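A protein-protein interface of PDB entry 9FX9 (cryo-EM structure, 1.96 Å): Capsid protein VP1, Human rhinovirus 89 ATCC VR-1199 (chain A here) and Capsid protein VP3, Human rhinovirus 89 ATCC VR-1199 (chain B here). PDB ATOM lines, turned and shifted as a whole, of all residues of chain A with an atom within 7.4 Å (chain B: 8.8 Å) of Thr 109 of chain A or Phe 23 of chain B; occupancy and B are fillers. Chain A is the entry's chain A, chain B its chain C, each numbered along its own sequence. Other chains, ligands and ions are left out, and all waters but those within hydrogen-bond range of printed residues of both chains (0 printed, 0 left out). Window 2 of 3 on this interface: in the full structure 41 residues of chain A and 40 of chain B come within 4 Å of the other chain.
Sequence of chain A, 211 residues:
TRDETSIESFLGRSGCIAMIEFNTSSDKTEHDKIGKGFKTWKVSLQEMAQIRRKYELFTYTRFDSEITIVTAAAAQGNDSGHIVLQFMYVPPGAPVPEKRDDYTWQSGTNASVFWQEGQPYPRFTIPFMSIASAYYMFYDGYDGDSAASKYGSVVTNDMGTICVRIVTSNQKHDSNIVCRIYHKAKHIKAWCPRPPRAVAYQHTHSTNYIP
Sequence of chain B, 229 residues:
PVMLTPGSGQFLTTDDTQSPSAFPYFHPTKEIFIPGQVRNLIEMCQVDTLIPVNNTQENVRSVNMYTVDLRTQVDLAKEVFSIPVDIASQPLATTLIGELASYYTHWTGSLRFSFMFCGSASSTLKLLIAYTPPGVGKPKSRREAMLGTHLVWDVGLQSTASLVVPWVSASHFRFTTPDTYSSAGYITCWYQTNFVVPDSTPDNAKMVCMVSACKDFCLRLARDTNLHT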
ATOM      1  N   MET A  88      20.279 -14.695   8.033  1.00  0.00           N
ATOM      2  CA  MET A  88      19.896 -14.738   6.635  1.00  0.00           C
ATOM      3  C   MET A  88      21.059 -15.197   5.765  1.00  0.00           C
ATOM      4  O   MET A  88      22.141 -14.617   5.803  1.00  0.00           O
ATOM      5  CB  MET A  88      19.342 -13.374   6.232  1.00  0.00           C
ATOM      6  CG  MET A  88      18.947 -13.350   4.758  1.00  0.00           C
ATOM      7  SD  MET A  88      18.050 -11.867   4.271  1.00  0.00           S
ATOM      8  CE  MET A  88      19.343 -10.615   4.403  1.00  0.00           C
ATOM      9  N   TYR A  89      20.821 -16.216   4.950  1.00  0.00           N
ATOM     10  CA  TYR A  89      21.716 -16.617   3.884  1.00  0.00           C
ATOM     11  C   TYR A  89      21.331 -15.910   2.588  1.00  0.00           C
ATOM     12  O   TYR A  89      20.238 -16.115   2.058  1.00  0.00           O
ATOM     13  CB  TYR A  89      21.689 -18.134   3.688  1.00  0.00           C
ATOM     14  CG  TYR A  89      22.990 -18.580   3.071  1.00  0.00           C
ATOM     15  CD1 TYR A  89      23.195 -18.584   1.679  1.00  0.00           C
ATOM     16  CD2 TYR A  89      24.045 -18.860   3.947  1.00  0.00           C
ATOM     17  CE1 TYR A  89      24.484 -18.828   1.164  1.00  0.00           C
ATOM     18  CE2 TYR A  89      25.323 -19.115   3.440  1.00  0.00           C
ATOM     19  CZ  TYR A  89      25.553 -19.062   2.056  1.00  0.00           C
ATOM     20  OH  TYR A  89      26.820 -19.249   1.618  1.00  0.00           O
ATOM     21  N   VAL A  90      22.238 -15.099   2.062  1.00  0.00           N
ATOM     22  CA  VAL A  90      22.101 -14.441   0.764  1.00  0.00           C
ATOM     23  C   VAL A  90      22.911 -15.258  -0.243  1.00  0.00           C
ATOM     24  O   VAL A  90      24.129 -15.354  -0.085  1.00  0.00           O
ATOM     25  CB  VAL A  90      22.604 -12.991   0.847  1.00  0.00           C
ATOM     26  CG1 VAL A  90      22.487 -12.280  -0.498  1.00  0.00           C
ATOM     27  CG2 VAL A  90      21.812 -12.183   1.874  1.00  0.00           C
ATOM     28  N   PRO A  91      22.288 -15.882  -1.256  1.00  0.00           N
ATOM     29  CA  PRO A  91      23.000 -16.720  -2.213  1.00  0.00           C
ATOM     30  C   PRO A  91      23.922 -15.898  -3.133  1.00  0.00           C
ATOM     31  O   PRO A  91      23.777 -14.677  -3.218  1.00  0.00           O
ATOM     32  CB  PRO A  91      21.904 -17.460  -2.984  1.00  0.00           C
ATOM     33  CG  PRO A  91      20.705 -16.531  -2.902  1.00  0.00           C
ATOM     34  CD  PRO A  91      20.867 -15.862  -1.543  1.00  0.00           C
ATOM     35  N   PRO A  92      24.867 -16.536  -3.845  1.00  0.00           N
ATOM     36  CA  PRO A  92      25.753 -15.861  -4.788  1.00  0.00           C
ATOM     37  C   PRO A  92      25.025 -14.930  -5.764  1.00  0.00           C
ATOM     38  O   PRO A  92      24.029 -15.310  -6.380  1.00  0.00           O
ATOM     39  CB  PRO A  92      26.470 -16.977  -5.543  1.00  0.00           C
ATOM     40  CG  PRO A  92      26.509 -18.098  -4.521  1.00  0.00           C
ATOM     41  CD  PRO A  92      25.174 -17.956  -3.800  1.00  0.00           C
ATOM     42  N   ALA A  94      23.083 -12.352  -5.285  1.00  0.00           N
ATOM     43  CA  ALA A  94      21.966 -11.599  -4.710  1.00  0.00           C
ATOM     44  C   ALA A  94      22.466 -10.392  -3.882  1.00  0.00           C
ATOM     45  O   ALA A  94      23.589 -10.415  -3.379  1.00  0.00           O
ATOM     46  CB  ALA A  94      21.099 -12.567  -3.903  1.00  0.00           C
ATOM     47  N   THR A 104      16.237  -6.195   1.691  1.00  0.00           N
ATOM     48  CA  THR A 104      16.882  -7.501   1.497  1.00  0.00           C
ATOM     49  C   THR A 104      16.535  -8.518   2.592  1.00  0.00           C
ATOM     50  O   THR A 104      16.412  -9.703   2.293  1.00  0.00           O
ATOM     51  CB  THR A 104      18.405  -7.337   1.397  1.00  0.00           C
ATOM     52  OG1 THR A 104      18.877  -6.578   2.475  1.00  0.00           O
ATOM     53  CG2 THR A 104      18.812  -6.615   0.121  1.00  0.00           C
ATOM     54  N   GLN A 106      13.588  -8.889   3.930  1.00  0.00           N
ATOM     55  CA  GLN A 106      12.213  -9.319   3.662  1.00  0.00           C
ATOM     56  C   GLN A 106      12.100 -10.202   2.406  1.00  0.00           C
ATOM     57  O   GLN A 106      11.052 -10.806   2.169  1.00  0.00           O
ATOM     58  CB  GLN A 106      11.313  -8.082   3.521  1.00  0.00           C
ATOM     59  CG  GLN A 106      11.325  -7.167   4.759  1.00  0.00           C
ATOM     60  CD  GLN A 106      10.490  -5.904   4.570  1.00  0.00           C
ATOM     61  OE1 GLN A 106       9.721  -5.750   3.634  1.00  0.00           O
ATOM     62  NE2 GLN A 106      10.598  -4.945   5.461  1.00  0.00           N
ATOM     63  N   SER A 107      13.149 -10.277   1.584  1.00  0.00           N
ATOM     64  CA  SER A 107      13.126 -11.005   0.313  1.00  0.00           C
ATOM     65  C   SER A 107      12.910 -12.505   0.511  1.00  0.00           C
ATOM     66  O   SER A 107      13.700 -13.177   1.169  1.00  0.00           O
ATOM     67  CB  SER A 107      14.423 -10.761  -0.462  1.00  0.00           C
ATOM     68  OG  SER A 107      14.421 -11.498  -1.673  1.00  0.00           O
ATOM     69  N   GLY A 108      11.874 -13.055  -0.121  1.00  0.00           N
ATOM     70  CA  GLY A 108      11.577 -14.490  -0.107  1.00  0.00           C
ATOM     71  C   GLY A 108      12.573 -15.350  -0.893  1.00  0.00           C
ATOM     72  O   GLY A 108      12.510 -16.575  -0.826  1.00  0.00           O
ATOM     73  N   THR A 109      13.486 -14.733  -1.648  1.00  0.00           N
ATOM     74  CA  THR A 109      14.565 -15.427  -2.375  1.00  0.00           C
ATOM     75  C   THR A 109      15.793 -15.698  -1.497  1.00  0.00           C
ATOM     76  O   THR A 109      16.539 -16.632  -1.774  1.00  0.00           O
ATOM     77  CB  THR A 109      14.929 -14.630  -3.636  1.00  0.00           C
ATOM     78  OG1 THR A 109      13.820 -14.649  -4.508  1.00  0.00           O
ATOM     79  CG2 THR A 109      16.098 -15.185  -4.447  1.00  0.00           C
ATOM     80  N   ASN A 110      15.998 -14.946  -0.413  1.00  0.00           N
ATOM     81  CA  ASN A 110      16.979 -15.291   0.615  1.00  0.00           C
ATOM     82  C   ASN A 110      16.406 -16.347   1.571  1.00  0.00           C
ATOM     83  O   ASN A 110      15.202 -16.379   1.822  1.00  0.00           O
ATOM     84  CB  ASN A 110      17.416 -14.026   1.374  1.00  0.00           C
ATOM     85  CG  ASN A 110      18.088 -12.994   0.493  1.00  0.00           C
ATOM     86  OD1 ASN A 110      18.688 -13.304  -0.518  1.00  0.00           O
ATOM     87  ND2 ASN A 110      18.024 -11.735   0.836  1.00  0.00           N
ATOM     88  N   ALA A 111      17.250 -17.191   2.153  1.00  0.00           N
ATOM     89  CA  ALA A 111      16.830 -18.107   3.209  1.00  0.00           C
ATOM     90  C   ALA A 111      17.065 -17.467   4.577  1.00  0.00           C
ATOM     91  O   ALA A 111      18.199 -17.152   4.913  1.00  0.00           O
ATOM     92  CB  ALA A 111      17.597 -19.416   3.059  1.00  0.00           C
ATOM     93  N   SER A 112      16.023 -17.278   5.381  1.00  0.00           N
ATOM     94  CA  SER A 112      16.145 -16.771   6.754  1.00  0.00           C
ATOM     95  C   SER A 112      15.750 -17.825   7.775  1.00  0.00           C
ATOM     96  O   SER A 112      14.759 -18.528   7.602  1.00  0.00           O
ATOM     97  CB  SER A 112      15.303 -15.519   6.992  1.00  0.00           C
ATOM     98  OG  SER A 112      15.829 -14.427   6.281  1.00  0.00           O
ATOM     99  N   PHE A 124      20.842 -25.149   9.064  1.00  0.00           N
ATOM    100  CA  PHE A 124      20.336 -25.314   7.701  1.00  0.00           C
ATOM    101  C   PHE A 124      21.450 -25.800   6.771  1.00  0.00           C
ATOM    102  O   PHE A 124      22.627 -25.562   7.020  1.00  0.00           O
ATOM    103  CB  PHE A 124      19.711 -23.996   7.216  1.00  0.00           C
ATOM    104  CG  PHE A 124      20.619 -22.782   7.284  1.00  0.00           C
ATOM    105  CD1 PHE A 124      21.457 -22.460   6.202  1.00  0.00           C
ATOM    106  CD2 PHE A 124      20.632 -21.967   8.429  1.00  0.00           C
ATOM    107  CE1 PHE A 124      22.293 -21.331   6.266  1.00  0.00           C
ATOM    108  CE2 PHE A 124      21.466 -20.841   8.494  1.00  0.00           C
ATOM    109  CZ  PHE A 124      22.299 -20.524   7.412  1.00  0.00           C
ATOM    110  N   THR A 125      21.095 -26.469   5.680  1.00  0.00           N
ATOM    111  CA  THR A 125      22.047 -26.866   4.636  1.00  0.00           C
ATOM    112  C   THR A 125      21.890 -25.965   3.423  1.00  0.00           C
ATOM    113  O   THR A 125      20.807 -25.905   2.846  1.00  0.00           O
ATOM    114  CB  THR A 125      21.867 -28.335   4.238  1.00  0.00           C
ATOM    115  OG1 THR A 125      22.217 -29.160   5.321  1.00  0.00           O
ATOM    116  CG2 THR A 125      22.772 -28.766   3.087  1.00  0.00           C
ATOM    117  N   ILE A 126      22.953 -25.295   2.994  1.00  0.00           N
ATOM    118  CA  ILE A 126      22.989 -24.659   1.678  1.00  0.00           C
ATOM    119  C   ILE A 126      23.425 -25.704   0.636  1.00  0.00           C
ATOM    120  O   ILE A 126      24.383 -26.442   0.884  1.00  0.00           O
ATOM    121  CB  ILE A 126      23.840 -23.375   1.666  1.00  0.00           C
ATOM    122  CG1 ILE A 126      25.352 -23.637   1.672  1.00  0.00           C
ATOM    123  CG2 ILE A 126      23.433 -22.459   2.831  1.00  0.00           C
ATOM    124  CD1 ILE A 126      26.199 -22.365   1.589  1.00  0.00           C
ATOM    125  N   PRO A 127      22.746 -25.822  -0.515  1.00  0.00           N
ATOM    126  CA  PRO A 127      23.217 -26.672  -1.606  1.00  0.00           C
ATOM    127  C   PRO A 127      24.565 -26.188  -2.152  1.00  0.00           C
ATOM    128  O   PRO A 127      24.970 -25.053  -1.917  1.00  0.00           O
ATOM    129  CB  PRO A 127      22.144 -26.588  -2.696  1.00  0.00           C
ATOM    130  CG  PRO A 127      20.927 -26.008  -1.991  1.00  0.00           C
ATOM    131  CD  PRO A 127      21.524 -25.145  -0.892  1.00  0.00           C
ATOM    132  N   MET A 129      26.165 -24.165  -4.544  1.00  0.00           N
ATOM    133  CA  MET A 129      25.557 -23.000  -5.217  1.00  0.00           C
ATOM    134  C   MET A 129      26.207 -22.579  -6.542  1.00  0.00           C
ATOM    135  O   MET A 129      25.617 -21.818  -7.309  1.00  0.00           O
ATOM    136  CB  MET A 129      25.624 -21.785  -4.278  1.00  0.00           C
ATOM    137  CG  MET A 129      24.632 -21.818  -3.122  1.00  0.00           C
ATOM    138  SD  MET A 129      22.926 -21.546  -3.640  1.00  0.00           S
ATOM    139  CE  MET A 129      22.224 -21.080  -2.054  1.00  0.00           C
ATOM    140  N   PRO B  20      17.267 -29.127   7.380  1.00  0.00           N
ATOM    141  CA  PRO B  20      16.489 -28.620   6.262  1.00  0.00           C
ATOM    142  C   PRO B  20      17.388 -27.960   5.215  1.00  0.00           C
ATOM    143  O   PRO B  20      18.310 -27.208   5.540  1.00  0.00           O
ATOM    144  CB  PRO B  20      15.473 -27.652   6.873  1.00  0.00           C
ATOM    145  CG  PRO B  20      16.166 -27.164   8.140  1.00  0.00           C
ATOM    146  CD  PRO B  20      16.958 -28.386   8.594  1.00  0.00           C
ATOM    147  N   SER B  21      17.101 -28.204   3.939  1.00  0.00           N
ATOM    148  CA  SER B  21      17.689 -27.407   2.863  1.00  0.00           C
ATOM    149  C   SER B  21      17.186 -25.972   2.955  1.00  0.00           C
ATOM    150  O   SER B  21      15.983 -25.728   3.030  1.00  0.00           O
ATOM    151  CB  SER B  21      17.377 -28.003   1.490  1.00  0.00           C
ATOM    152  OG  SER B  21      17.941 -27.184   0.484  1.00  0.00           O
ATOM    153  N   ALA B  22      18.102 -25.009   2.945  1.00  0.00           N
ATOM    154  CA  ALA B  22      17.770 -23.591   2.895  1.00  0.00           C
ATOM    155  C   ALA B  22      17.117 -23.203   1.556  1.00  0.00           C
ATOM    156  O   ALA B  22      16.383 -22.221   1.495  1.00  0.00           O
ATOM    157  CB  ALA B  22      19.064 -22.816   3.149  1.00  0.00           C
ATOM    158  N   PHE B  23      17.353 -23.975   0.495  1.00  0.00           N
ATOM    159  CA  PHE B  23      16.912 -23.671  -0.864  1.00  0.00           C
ATOM    160  C   PHE B  23      16.349 -24.927  -1.540  1.00  0.00           C
ATOM    161  O   PHE B  23      17.014 -25.525  -2.383  1.00  0.00           O
ATOM    162  CB  PHE B  23      18.067 -23.036  -1.663  1.00  0.00           C
ATOM    163  CG  PHE B  23      18.614 -21.761  -1.060  1.00  0.00           C
ATOM    164  CD1 PHE B  23      18.052 -20.519  -1.403  1.00  0.00           C
ATOM    165  CD2 PHE B  23      19.673 -21.809  -0.139  1.00  0.00           C
ATOM    166  CE1 PHE B  23      18.550 -19.340  -0.826  1.00  0.00           C
ATOM    167  CE2 PHE B  23      20.168 -20.630   0.444  1.00  0.00           C
ATOM    168  CZ  PHE B  23      19.605 -19.392   0.095  1.00  0.00           C
ATOM    169  N   PRO B  24      15.117 -25.355  -1.209  1.00  0.00           N
ATOM    170  CA  PRO B  24      14.366 -26.253  -2.077  1.00  0.00           C
ATOM    171  C   PRO B  24      14.054 -25.532  -3.400  1.00  0.00           C
ATOM    172  O   PRO B  24      14.261 -24.326  -3.530  1.00  0.00           O
ATOM    173  CB  PRO B  24      13.119 -26.618  -1.276  1.00  0.00           C
ATOM    174  CG  PRO B  24      12.857 -25.361  -0.454  1.00  0.00           C
ATOM    175  CD  PRO B  24      14.259 -24.832  -0.159  1.00  0.00           C
ATOM    176  N   TYR B  25      13.580 -26.258  -4.407  1.00  0.00           N
ATOM    177  CA  TYR B  25      13.425 -25.793  -5.799  1.00  0.00           C
ATOM    178  C   TYR B  25      14.739 -25.500  -6.543  1.00  0.00           C
ATOM    179  O   TYR B  25      14.806 -25.722  -7.754  1.00  0.00           O
ATOM    180  CB  TYR B  25      12.464 -24.596  -5.917  1.00  0.00           C
ATOM    181  CG  TYR B  25      11.169 -24.702  -5.137  1.00  0.00           C
ATOM    182  CD1 TYR B  25      10.186 -25.620  -5.537  1.00  0.00           C
ATOM    183  CD2 TYR B  25      10.935 -23.851  -4.043  1.00  0.00           C
ATOM    184  CE1 TYR B  25       8.961 -25.688  -4.849  1.00  0.00           C
ATOM    185  CE2 TYR B  25       9.710 -23.912  -3.354  1.00  0.00           C
ATOM    186  CZ  TYR B  25       8.718 -24.826  -3.762  1.00  0.00           C
ATOM    187  OH  TYR B  25       7.524 -24.879  -3.119  1.00  0.00           O
ATOM    188  N   PHE B  26      15.798 -25.057  -5.869  1.00  0.00           N
ATOM    189  CA  PHE B  26      17.121 -24.922  -6.478  1.00  0.00           C
ATOM    190  C   PHE B  26      17.718 -26.290  -6.824  1.00  0.00           C
ATOM    191  O   PHE B  26      17.837 -27.162  -5.965  1.00  0.00           O
ATOM    192  CB  PHE B  26      18.060 -24.133  -5.560  1.00  0.00           C
ATOM    193  CG  PHE B  26      19.457 -23.981  -6.126  1.00  0.00           C
ATOM    194  CD1 PHE B  26      19.716 -23.015  -7.117  1.00  0.00           C
ATOM    195  CD2 PHE B  26      20.494 -24.823  -5.699  1.00  0.00           C
ATOM    196  CE1 PHE B  26      21.002 -22.888  -7.665  1.00  0.00           C
ATOM    197  CE2 PHE B  26      21.786 -24.683  -6.231  1.00  0.00           C
ATOM    198  CZ  PHE B  26      22.040 -23.721  -7.218  1.00  0.00           C
ATOM    199  N   HIS B  27      18.127 -26.467  -8.074  1.00  0.00           N
ATOM    200  CA  HIS B  27      18.859 -27.648  -8.525  1.00  0.00           C
ATOM    201  C   HIS B  27      20.326 -27.252  -8.742  1.00  0.00           C
ATOM    202  O   HIS B  27      20.594 -26.409  -9.598  1.00  0.00           O
ATOM    203  CB  HIS B  27      18.212 -28.195  -9.805  1.00  0.00           C
ATOM    204  CG  HIS B  27      16.842 -28.788  -9.587  1.00  0.00           C
ATOM    205  ND1 HIS B  27      15.690 -28.118  -9.243  1.00  0.00           N
ATOM    206  CD2 HIS B  27      16.532 -30.119  -9.606  1.00  0.00           C
ATOM    207  CE1 HIS B  27      14.709 -29.016  -9.079  1.00  0.00           C
ATOM    208  NE2 HIS B  27      15.174 -30.258  -9.294  1.00  0.00           N
ATOM    209  N   PRO B  28      21.285 -27.828  -7.996  1.00  0.00           N
ATOM    210  CA  PRO B  28      22.708 -27.559  -8.176  1.00  0.00           C
ATOM    211  C   PRO B  28      23.195 -27.824  -9.598  1.00  0.00           C
ATOM    212  O   PRO B  28      22.684 -28.709 -10.284  1.00  0.00           O
ATOM    213  CB  PRO B  28      23.434 -28.478  -7.190  1.00  0.00           C
ATOM    214  CG  PRO B  28      22.404 -28.686  -6.091  1.00  0.00           C
ATOM    215  CD  PRO B  28      21.090 -28.711  -6.860  1.00  0.00           C
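The backbone carbonyl oxygen of Ala 111 of chain A sits at hydrogen-bond distance from the backbone NH of Tyr 89 of chain A (2.8 Å).
The side-chain hydroxyl (OG) of Ser 107 of chain A sits close to the backbone NH (N) of Thr 109 of chain A (3.4 Å).
The backbone NH of Phe 23 of chain B sits close to the side-chain hydroxyl of Ser 21 of chain B.
Of the 9 printed residues of chain B, 6 touch a printed residue of chain A.
Printed residues of chain B that touch a printed residue of chain A: Pro 20, Ser 21, Ala 22, Phe 23, Phe 26 and Pro 28.
Of the 19 printed residues of chain A, 7 touch a printed residue of chain B.
Hydrophobic or aromatic side chains of chain A that line the printed part of chain B: Tyr 89, Ala 111, Phe 124, Pro 127 and Met 129.
N of Thr 125 of chain A lies within hydrogen-bond range of O of Pro 20 of chain B (2.9 Å).
The backbone carbonyl oxygen of Thr 125 of chain A lies within hydrogen-bond range of the backbone NH of Ala 22 of chain B (2.9 Å).
Of the printed residues of chain B, Tyr 89 of chain A touches Phe 23.
Thr 104 of chain A touches none of the printed residues of chain B.
No residue of chain B comes within 4 Å of Gly 108 of chain A.
Thr 109 of chain A touches just one residue of chain B: Phe 23.
Printed residues of chain B within 4 Å of Pro 127 of chain A: Phe 23 (3.9 Å), Phe 26 (3.9 Å) and Pro 28 (3.999 Å).
Printed residues of chain B within 4 Å of Met 129 of chain A: Phe 23.
Phe 23 of chain B touches five residues of chain A.
Among the printed residues, pairs that only touch across the chains: Tyr 89 of chain A with Phe 23 of chain B (3.9 Å), Thr 109 of chain A with Phe 23 of chain B (3.5 Å), Ala 111 of chain A with Ala 22 of chain B (3.4 Å), Ala 111 of chain A with Phe 23 of chain B (3.6 Å), Phe 124 of chain A with Pro 20 of chain B (3.5 Å), Phe 124 of chain A with Ala 22 of chain B (3.9 Å), Thr 125 of chain A with Ser 21 of chain B (3.5 Å), Pro 127 of chain A with Phe 23 of chain B (3.9 Å), Pro 127 of chain A with Phe 26 of chain B (3.9 Å), Pro 127 of chain A with Pro 28 of chain B (3.999 Å) and Met 129 of chain A with Phe 23 of chain B (3.3 Å).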
